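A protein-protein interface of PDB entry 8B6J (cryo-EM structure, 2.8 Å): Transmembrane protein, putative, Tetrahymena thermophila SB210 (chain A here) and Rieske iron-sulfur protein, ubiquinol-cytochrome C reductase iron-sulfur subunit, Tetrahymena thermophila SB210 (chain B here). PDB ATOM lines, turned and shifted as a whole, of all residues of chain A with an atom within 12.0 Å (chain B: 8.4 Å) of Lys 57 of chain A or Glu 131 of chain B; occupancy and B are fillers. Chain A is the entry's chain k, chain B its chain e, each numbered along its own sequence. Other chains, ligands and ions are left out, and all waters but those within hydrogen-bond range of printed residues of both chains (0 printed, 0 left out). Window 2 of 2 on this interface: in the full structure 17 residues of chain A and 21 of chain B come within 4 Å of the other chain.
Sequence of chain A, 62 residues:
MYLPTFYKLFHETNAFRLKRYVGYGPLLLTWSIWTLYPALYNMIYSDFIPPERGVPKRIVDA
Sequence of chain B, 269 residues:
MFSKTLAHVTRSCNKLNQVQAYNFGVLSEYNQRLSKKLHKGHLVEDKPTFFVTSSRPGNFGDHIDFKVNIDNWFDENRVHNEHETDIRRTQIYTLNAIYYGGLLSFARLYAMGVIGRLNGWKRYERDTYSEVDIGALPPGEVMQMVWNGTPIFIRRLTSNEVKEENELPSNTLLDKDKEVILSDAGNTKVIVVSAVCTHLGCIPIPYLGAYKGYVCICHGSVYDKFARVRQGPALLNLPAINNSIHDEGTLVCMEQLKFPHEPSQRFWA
The side-chain hydroxyl (OH) of Tyr 129 of chain B sits at hydrogen-bond distance from the side-chain carboxylate (OE2) of Glu 131 of chain B. O of Cys 253 of chain B is in hydrogen-bond range of N of Ser 244 of chain B, 2.9 Å away. A ring nitrogen (ND1) of His 246 of chain B lies within hydrogen-bond range of the side-chain sulfur (SG) of Cys 253 of chain B (3.1 Å).
Printed residues of chain B within 4 Å of Gly 54 of chain A: Ser 244. Of the printed residues of chain B, Val 55 of chain A touches Ser 244 (3.4 Å), His 246 (3.2 Å), Cys 253 (3.2 Å) and Glu 255 (3.6 Å). Printed residues of chain B within 4 Å of Lys 57 of chain A: Tyr 129, Glu 131 and His 246. Of the printed residues of chain B, Arg 58 of chain A touches Tyr 129 (3.2 Å). Tyr 129 of chain B touches just these residues of chain A: Pro 56, Lys 57 and Arg 58. No residue of chain A comes within 4 Å of Ser 130 of chain B. Of the printed residues of chain A, Glu 131 of chain B touches Lys 57. No residue of chain A comes within 4 Å of Val 132 of chain B. Leu 251 of chain B touches none of the printed residues of chain A. No residue of chain A comes within 4 Å of Val 252 of chain B. Cys 253 of chain B touches two residues of chain A. No residue of chain A comes within 4 Å of Met 254 of chain B.
CA of Gly 54 of chain A touches OG of Ser 244 of chain B, at 3.8 Å. CE1 of His 246 of chain B touches O of Val 55 of chain A, 3.2 Å away. Cys 253 of chain B touches Val 55 of chain A (O to CG2, 3.2 Å). CB of Glu 255 of chain B touches CG1 of Val 55 of chain A, at 3.6 Å. O of Pro 56 of chain A touches CE1 of Tyr 129 of chain B, at 3.7 Å. Cys 253 of chain B touches Pro 56 of chain A. CD of Pro 56 of chain A touches OE1 of Glu 255 of chain B, at 3.6 Å. O of Lys 57 of chain A touches OE2 of Glu 131 of chain B, 3.9 Å away. Lys 57 of chain A touches His 246 of chain B. Tyr 129 of chain B touches Arg 58 of chain A.
N of Val 55 of chain A sits at hydrogen-bond distance from OG of Ser 244 of chain B (3.4 Å). O of Lys 57 of chain A lies within hydrogen-bond range of OH of Tyr 129 of chain B (2.9 Å).
Of the 21 printed residues of chain B, 6 touch a printed residue of chain A. Printed residues of chain B that touch a printed residue of chain A: Tyr 129, Glu 131, Ser 244, His 246, Cys 253 and Glu 255. Among the printed residues, no Asp or Glu carboxylate lies within 4 Å of a Lys or Arg side-chain nitrogen of the other chain.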
ATOM      1  N   ARG A  53     -15.463  16.865  20.903  1.00  0.00           N
ATOM      2  CA  ARG A  53     -16.217  15.957  21.763  1.00  0.00           C
ATOM      3  C   ARG A  53     -17.550  16.611  22.104  1.00  0.00           C
ATOM      4  O   ARG A  53     -17.626  17.481  22.975  1.00  0.00           O
ATOM      5  CB  ARG A  53     -15.424  15.621  23.021  1.00  0.00           C
ATOM      6  CG  ARG A  53     -14.158  14.827  22.758  1.00  0.00           C
ATOM      7  CD  ARG A  53     -13.481  14.421  24.054  1.00  0.00           C
ATOM      8  NE  ARG A  53     -12.270  13.645  23.820  1.00  0.00           N
ATOM      9  CZ  ARG A  53     -11.507  13.138  24.779  1.00  0.00           C
ATOM     10  NH1 ARG A  53     -11.802  13.303  26.058  1.00  0.00           N
ATOM     11  NH2 ARG A  53     -10.420  12.447  24.446  1.00  0.00           N
ATOM     12  N   GLY A  54     -18.603  16.192  21.411  1.00  0.00           N
ATOM     13  CA  GLY A  54     -19.943  16.672  21.683  1.00  0.00           C
ATOM     14  C   GLY A  54     -20.975  15.858  20.934  1.00  0.00           C
ATOM     15  O   GLY A  54     -20.687  15.332  19.855  1.00  0.00           O
ATOM     16  N   VAL A  55     -22.179  15.741  21.488  1.00  0.00           N
ATOM     17  CA  VAL A  55     -23.238  14.959  20.854  1.00  0.00           C
ATOM     18  C   VAL A  55     -24.530  15.768  20.861  1.00  0.00           C
ATOM     19  O   VAL A  55     -24.754  16.569  21.780  1.00  0.00           O
ATOM     20  CB  VAL A  55     -23.423  13.604  21.556  1.00  0.00           C
ATOM     21  CG1 VAL A  55     -22.146  12.787  21.468  1.00  0.00           C
ATOM     22  CG2 VAL A  55     -23.827  13.801  23.004  1.00  0.00           C
ATOM     23  N   PRO A  56     -25.406  15.591  19.876  1.00  0.00           N
ATOM     24  CA  PRO A  56     -26.641  16.378  19.835  1.00  0.00           C
ATOM     25  C   PRO A  56     -27.590  16.000  20.961  1.00  0.00           C
ATOM     26  O   PRO A  56     -27.558  14.891  21.500  1.00  0.00           O
ATOM     27  CB  PRO A  56     -27.237  16.036  18.466  1.00  0.00           C
ATOM     28  CG  PRO A  56     -26.701  14.685  18.155  1.00  0.00           C
ATOM     29  CD  PRO A  56     -25.324  14.638  18.755  1.00  0.00           C
ATOM     30  N   LYS A  57     -28.452  16.956  21.311  1.00  0.00           N
ATOM     31  CA  LYS A  57     -29.416  16.725  22.381  1.00  0.00           C
ATOM     32  C   LYS A  57     -30.352  15.571  22.039  1.00  0.00           C
ATOM     33  O   LYS A  57     -30.676  14.748  22.904  1.00  0.00           O
ATOM     34  CB  LYS A  57     -30.213  18.002  22.650  1.00  0.00           C
ATOM     35  CG  LYS A  57     -30.973  18.530  21.442  1.00  0.00           C
ATOM     36  CD  LYS A  57     -31.661  19.849  21.750  1.00  0.00           C
ATOM     37  CE  LYS A  57     -32.406  20.381  20.537  1.00  0.00           C
ATOM     38  NZ  LYS A  57     -33.088  21.672  20.824  1.00  0.00           N
ATOM     39  N   ARG A  58     -30.799  15.495  20.790  1.00  0.00           N
ATOM     40  CA  ARG A  58     -31.689  14.424  20.360  1.00  0.00           C
ATOM     41  C   ARG A  58     -30.963  13.084  20.360  1.00  0.00           C
ATOM     42  O   ARG A  58     -30.938  12.382  19.350  1.00  0.00           O
ATOM     43  CB  ARG A  58     -32.245  14.716  18.965  1.00  0.00           C
ATOM     44  CG  ARG A  58     -33.056  15.996  18.876  1.00  0.00           C
ATOM     45  CD  ARG A  58     -33.559  16.234  17.463  1.00  0.00           C
ATOM     46  NE  ARG A  58     -34.297  17.485  17.349  1.00  0.00           N
ATOM     47  CZ  ARG A  58     -34.809  17.954  16.218  1.00  0.00           C
ATOM     48  NH1 ARG A  58     -34.679  17.297  15.077  1.00  0.00           N
ATOM     49  NH2 ARG A  58     -35.466  19.109  16.234  1.00  0.00           N
ATOM     50  N   THR B 128     -25.273   4.417  17.605  1.00  0.00           N
ATOM     51  CA  THR B 128     -24.815   4.048  18.937  1.00  0.00           C
ATOM     52  C   THR B 128     -25.327   5.016  19.996  1.00  0.00           C
ATOM     53  O   THR B 128     -24.918   4.918  21.158  1.00  0.00           O
ATOM     54  CB  THR B 128     -23.284   3.989  18.986  1.00  0.00           C
ATOM     55  OG1 THR B 128     -22.856   3.755  20.333  1.00  0.00           O
ATOM     56  CG2 THR B 128     -22.681   5.288  18.482  1.00  0.00           C
ATOM     57  N   TYR B 129     -26.209   5.941  19.623  1.00  0.00           N
ATOM     58  CA  TYR B 129     -26.715   6.927  20.566  1.00  0.00           C
ATOM     59  C   TYR B 129     -27.460   6.244  21.705  1.00  0.00           C
ATOM     60  O   TYR B 129     -28.147   5.238  21.508  1.00  0.00           O
ATOM     61  CB  TYR B 129     -27.636   7.909  19.843  1.00  0.00           C
ATOM     62  CG  TYR B 129     -28.188   9.005  20.722  1.00  0.00           C
ATOM     63  CD1 TYR B 129     -27.504  10.201  20.885  1.00  0.00           C
ATOM     64  CD2 TYR B 129     -29.397   8.847  21.383  1.00  0.00           C
ATOM     65  CE1 TYR B 129     -28.007  11.207  21.686  1.00  0.00           C
ATOM     66  CE2 TYR B 129     -29.906   9.847  22.184  1.00  0.00           C
ATOM     67  CZ  TYR B 129     -29.208  11.024  22.333  1.00  0.00           C
ATOM     68  OH  TYR B 129     -29.715  12.022  23.133  1.00  0.00           O
ATOM     69  N   SER B 130     -27.312   6.796  22.906  1.00  0.00           N
ATOM     70  CA  SER B 130     -27.975   6.261  24.085  1.00  0.00           C
ATOM     71  C   SER B 130     -28.220   7.394  25.068  1.00  0.00           C
ATOM     72  O   SER B 130     -27.564   8.437  25.021  1.00  0.00           O
ATOM     73  CB  SER B 130     -27.144   5.154  24.742  1.00  0.00           C
ATOM     74  OG  SER B 130     -27.753   4.706  25.941  1.00  0.00           O
ATOM     75  N   GLU B 131     -29.179   7.177  25.964  1.00  0.00           N
ATOM     76  CA  GLU B 131     -29.514   8.136  27.006  1.00  0.00           C
ATOM     77  C   GLU B 131     -29.620   7.415  28.339  1.00  0.00           C
ATOM     78  O   GLU B 131     -30.218   6.338  28.426  1.00  0.00           O
ATOM     79  CB  GLU B 131     -30.826   8.861  26.694  1.00  0.00           C
ATOM     80  CG  GLU B 131     -30.778   9.683  25.420  1.00  0.00           C
ATOM     81  CD  GLU B 131     -32.037  10.497  25.200  1.00  0.00           C
ATOM     82  OE1 GLU B 131     -33.031  10.264  25.916  1.00  0.00           O
ATOM     83  OE2 GLU B 131     -32.030  11.373  24.309  1.00  0.00           O
ATOM     84  N   VAL B 132     -29.036   8.010  29.375  1.00  0.00           N
ATOM     85  CA  VAL B 132     -29.020   7.434  30.715  1.00  0.00           C
ATOM     86  C   VAL B 132     -29.608   8.449  31.684  1.00  0.00           C
ATOM     87  O   VAL B 132     -29.197   9.615  31.695  1.00  0.00           O
ATOM     88  CB  VAL B 132     -27.597   7.031  31.142  1.00  0.00           C
ATOM     89  CG1 VAL B 132     -27.619   6.371  32.511  1.00  0.00           C
ATOM     90  CG2 VAL B 132     -26.975   6.104  30.111  1.00  0.00           C
ATOM     91  N   ASP B 133     -30.568   8.006  32.493  1.00  0.00           N
ATOM     92  CA  ASP B 133     -31.162   8.856  33.518  1.00  0.00           C
ATOM     93  C   ASP B 133     -30.276   8.831  34.757  1.00  0.00           C
ATOM     94  O   ASP B 133     -30.073   7.773  35.361  1.00  0.00           O
ATOM     95  CB  ASP B 133     -32.575   8.381  33.850  1.00  0.00           C
ATOM     96  CG  ASP B 133     -33.337   9.368  34.717  1.00  0.00           C
ATOM     97  OD1 ASP B 133     -32.693  10.134  35.466  1.00  0.00           O
ATOM     98  OD2 ASP B 133     -34.585   9.379  34.651  1.00  0.00           O
ATOM     99  N   ILE B 134     -29.746   9.997  35.134  1.00  0.00           N
ATOM    100  CA  ILE B 134     -28.815  10.106  36.250  1.00  0.00           C
ATOM    101  C   ILE B 134     -29.189  11.214  37.222  1.00  0.00           C
ATOM    102  O   ILE B 134     -28.475  11.426  38.204  1.00  0.00           O
ATOM    103  CB  ILE B 134     -27.369  10.306  35.744  1.00  0.00           C
ATOM    104  CG1 ILE B 134     -27.090   9.353  34.576  1.00  0.00           C
ATOM    105  CG2 ILE B 134     -26.369  10.082  36.880  1.00  0.00           C
ATOM    106  CD1 ILE B 134     -25.693   9.441  34.016  1.00  0.00           C
ATOM    107  N   MET B 145     -22.903   1.178  34.006  1.00  0.00           N
ATOM    108  CA  MET B 145     -23.834   1.023  32.899  1.00  0.00           C
ATOM    109  C   MET B 145     -23.144   0.282  31.762  1.00  0.00           C
ATOM    110  O   MET B 145     -21.917   0.176  31.718  1.00  0.00           O
ATOM    111  CB  MET B 145     -24.352   2.379  32.405  1.00  0.00           C
ATOM    112  CG  MET B 145     -25.218   3.117  33.412  1.00  0.00           C
ATOM    113  SD  MET B 145     -26.756   2.253  33.789  1.00  0.00           S
ATOM    114  CE  MET B 145     -27.564   2.275  32.191  1.00  0.00           C
ATOM    115  N   VAL B 146     -23.951  -0.242  30.846  1.00  0.00           N
ATOM    116  CA  VAL B 146     -23.460  -0.953  29.672  1.00  0.00           C
ATOM    117  C   VAL B 146     -23.768  -0.101  28.450  1.00  0.00           C
ATOM    118  O   VAL B 146     -24.939   0.151  28.139  1.00  0.00           O
ATOM    119  CB  VAL B 146     -24.089  -2.349  29.546  1.00  0.00           C
ATOM    120  CG1 VAL B 146     -23.554  -3.064  28.315  1.00  0.00           C
ATOM    121  CG2 VAL B 146     -23.823  -3.166  30.801  1.00  0.00           C
ATOM    122  N   TRP B 147     -22.721   0.341  27.760  1.00  0.00           N
ATOM    123  CA  TRP B 147     -22.852   1.138  26.547  1.00  0.00           C
ATOM    124  C   TRP B 147     -22.001   0.502  25.460  1.00  0.00           C
ATOM    125  O   TRP B 147     -20.817   0.224  25.678  1.00  0.00           O
ATOM    126  CB  TRP B 147     -22.430   2.590  26.791  1.00  0.00           C
ATOM    127  CG  TRP B 147     -22.692   3.502  25.633  1.00  0.00           C
ATOM    128  CD1 TRP B 147     -23.909   3.913  25.173  1.00  0.00           C
ATOM    129  CD2 TRP B 147     -21.714   4.126  24.794  1.00  0.00           C
ATOM    130  NE1 TRP B 147     -23.750   4.750  24.096  1.00  0.00           N
ATOM    131  CE2 TRP B 147     -22.411   4.897  23.844  1.00  0.00           C
ATOM    132  CE3 TRP B 147     -20.318   4.106  24.751  1.00  0.00           C
ATOM    133  CZ2 TRP B 147     -21.760   5.640  22.864  1.00  0.00           C
ATOM    134  CZ3 TRP B 147     -19.673   4.844  23.778  1.00  0.00           C
ATOM    135  CH2 TRP B 147     -20.394   5.600  22.847  1.00  0.00           C
ATOM    136  N   ILE B 154     -20.308   6.156  35.788  1.00  0.00           N
ATOM    137  CA  ILE B 154     -20.811   7.523  35.853  1.00  0.00           C
ATOM    138  C   ILE B 154     -20.875   7.930  37.318  1.00  0.00           C
ATOM    139  O   ILE B 154     -21.454   7.212  38.141  1.00  0.00           O
ATOM    140  CB  ILE B 154     -22.192   7.660  35.189  1.00  0.00           C
ATOM    141  CG1 ILE B 154     -22.153   7.106  33.761  1.00  0.00           C
ATOM    142  CG2 ILE B 154     -22.627   9.120  35.200  1.00  0.00           C
ATOM    143  CD1 ILE B 154     -23.502   7.072  33.073  1.00  0.00           C
ATOM    144  N   SER B 244     -22.585  14.107  26.549  1.00  0.00           N
ATOM    145  CA  SER B 244     -23.004  15.469  26.845  1.00  0.00           C
ATOM    146  C   SER B 244     -24.212  15.419  27.767  1.00  0.00           C
ATOM    147  O   SER B 244     -24.844  14.373  27.942  1.00  0.00           O
ATOM    148  CB  SER B 244     -23.333  16.250  25.568  1.00  0.00           C
ATOM    149  OG  SER B 244     -22.177  16.438  24.771  1.00  0.00           O
ATOM    150  N   ILE B 245     -24.511  16.567  28.369  1.00  0.00           N
ATOM    151  CA  ILE B 245     -25.651  16.727  29.259  1.00  0.00           C
ATOM    152  C   ILE B 245     -26.510  17.861  28.721  1.00  0.00           C
ATOM    153  O   ILE B 245     -26.011  18.971  28.499  1.00  0.00           O
ATOM    154  CB  ILE B 245     -25.213  17.019  30.706  1.00  0.00           C
ATOM    155  CG1 ILE B 245     -23.888  16.323  31.035  1.00  0.00           C
ATOM    156  CG2 ILE B 245     -26.285  16.570  31.680  1.00  0.00           C
ATOM    157  CD1 ILE B 245     -23.915  14.820  30.889  1.00  0.00           C
ATOM    158  N   HIS B 246     -27.798  17.583  28.511  1.00  0.00           N
ATOM    159  CA  HIS B 246     -28.728  18.582  28.006  1.00  0.00           C
ATOM    160  C   HIS B 246     -29.993  18.719  28.838  1.00  0.00           C
ATOM    161  O   HIS B 246     -30.724  19.698  28.651  1.00  0.00           O
ATOM    162  CB  HIS B 246     -29.125  18.262  26.557  1.00  0.00           C
ATOM    163  CG  HIS B 246     -27.978  18.301  25.596  1.00  0.00           C
ATOM    164  ND1 HIS B 246     -27.156  17.217  25.373  1.00  0.00           N
ATOM    165  CD2 HIS B 246     -27.512  19.296  24.804  1.00  0.00           C
ATOM    166  CE1 HIS B 246     -26.236  17.541  24.483  1.00  0.00           C
ATOM    167  NE2 HIS B 246     -26.430  18.796  24.121  1.00  0.00           N
ATOM    168  N   ASP B 247     -30.275  17.785  29.747  1.00  0.00           N
ATOM    169  CA  ASP B 247     -31.456  17.841  30.599  1.00  0.00           C
ATOM    170  C   ASP B 247     -31.144  18.442  31.966  1.00  0.00           C
ATOM    171  O   ASP B 247     -31.767  18.071  32.966  1.00  0.00           O
ATOM    172  CB  ASP B 247     -32.059  16.447  30.755  1.00  0.00           C
ATOM    173  CG  ASP B 247     -33.529  16.486  31.120  1.00  0.00           C
ATOM    174  OD1 ASP B 247     -33.955  17.455  31.781  1.00  0.00           O
ATOM    175  OD2 ASP B 247     -34.260  15.547  30.743  1.00  0.00           O
ATOM    176  N   THR B 250     -30.226  15.877  34.528  1.00  0.00           N
ATOM    177  CA  THR B 250     -31.147  14.761  34.706  1.00  0.00           C
ATOM    178  C   THR B 250     -30.775  13.587  33.810  1.00  0.00           C
ATOM    179  O   THR B 250     -30.814  12.429  34.243  1.00  0.00           O
ATOM    180  CB  THR B 250     -32.580  15.216  34.424  1.00  0.00           C
ATOM    181  OG1 THR B 250     -32.917  16.306  35.292  1.00  0.00           O
ATOM    182  CG2 THR B 250     -33.561  14.073  34.646  1.00  0.00           C
ATOM    183  N   LEU B 251     -30.408  13.864  32.561  1.00  0.00           N
ATOM    184  CA  LEU B 251     -30.164  12.830  31.567  1.00  0.00           C
ATOM    185  C   LEU B 251     -28.853  13.111  30.848  1.00  0.00           C
ATOM    186  O   LEU B 251     -28.525  14.266  30.561  1.00  0.00           O
ATOM    187  CB  LEU B 251     -31.322  12.760  30.559  1.00  0.00           C
ATOM    188  CG  LEU B 251     -31.316  11.612  29.545  1.00  0.00           C
ATOM    189  CD1 LEU B 251     -32.733  11.332  29.072  1.00  0.00           C
ATOM    190  CD2 LEU B 251     -30.416  11.916  28.356  1.00  0.00           C
ATOM    191  N   VAL B 252     -28.113  12.045  30.555  1.00  0.00           N
ATOM    192  CA  VAL B 252     -26.831  12.122  29.868  1.00  0.00           C
ATOM    193  C   VAL B 252     -26.972  11.413  28.531  1.00  0.00           C
ATOM    194  O   VAL B 252     -27.388  10.249  28.484  1.00  0.00           O
ATOM    195  CB  VAL B 252     -25.702  11.487  30.702  1.00  0.00           C
ATOM    196  CG1 VAL B 252     -24.377  11.570  29.958  1.00  0.00           C
ATOM    197  CG2 VAL B 252     -25.611  12.154  32.065  1.00  0.00           C
ATOM    198  N   CYS B 253     -26.629  12.111  27.450  1.00  0.00           N
ATOM    199  CA  CYS B 253     -26.707  11.558  26.104  1.00  0.00           C
ATOM    200  C   CYS B 253     -25.301  11.203  25.639  1.00  0.00           C
ATOM    201  O   CYS B 253     -24.410  12.059  25.629  1.00  0.00           O
ATOM    202  CB  CYS B 253     -27.362  12.550  25.145  1.00  0.00           C
ATOM    203  SG  CYS B 253     -26.584  14.179  25.111  1.00  0.00           S
ATOM    204  N   MET B 254     -25.108   9.948  25.240  1.00  0.00           N
ATOM    205  CA  MET B 254     -23.802   9.429  24.865  1.00  0.00           C
ATOM    206  C   MET B 254     -23.843   8.900  23.440  1.00  0.00           C
ATOM    207  O   MET B 254     -24.831   8.290  23.020  1.00  0.00           O
ATOM    208  CB  MET B 254     -23.363   8.314  25.816  1.00  0.00           C
ATOM    209  CG  MET B 254     -23.207   8.759  27.259  1.00  0.00           C
ATOM    210  SD  MET B 254     -24.194   7.780  28.405  1.00  0.00           S
ATOM    211  CE  MET B 254     -23.545   6.141  28.096  1.00  0.00           C
ATOM    212  N   GLU B 255     -22.763   9.140  22.701  1.00  0.00           N
ATOM    213  CA  GLU B 255     -22.638   8.659  21.335  1.00  0.00           C
ATOM    214  C   GLU B 255     -21.160   8.612  20.982  1.00  0.00           C
ATOM    215  O   GLU B 255     -20.402   9.506  21.363  1.00  0.00           O
ATOM    216  CB  GLU B 255     -23.395   9.559  20.353  1.00  0.00           C
ATOM    217  CG  GLU B 255     -23.415   9.044  18.924  1.00  0.00           C
ATOM    218  CD  GLU B 255     -24.137   9.982  17.978  1.00  0.00           C
ATOM    219  OE1 GLU B 255     -24.368  11.148  18.357  1.00  0.00           O
ATOM    220  OE2 GLU B 255     -24.476   9.551  16.856  1.00  0.00           O
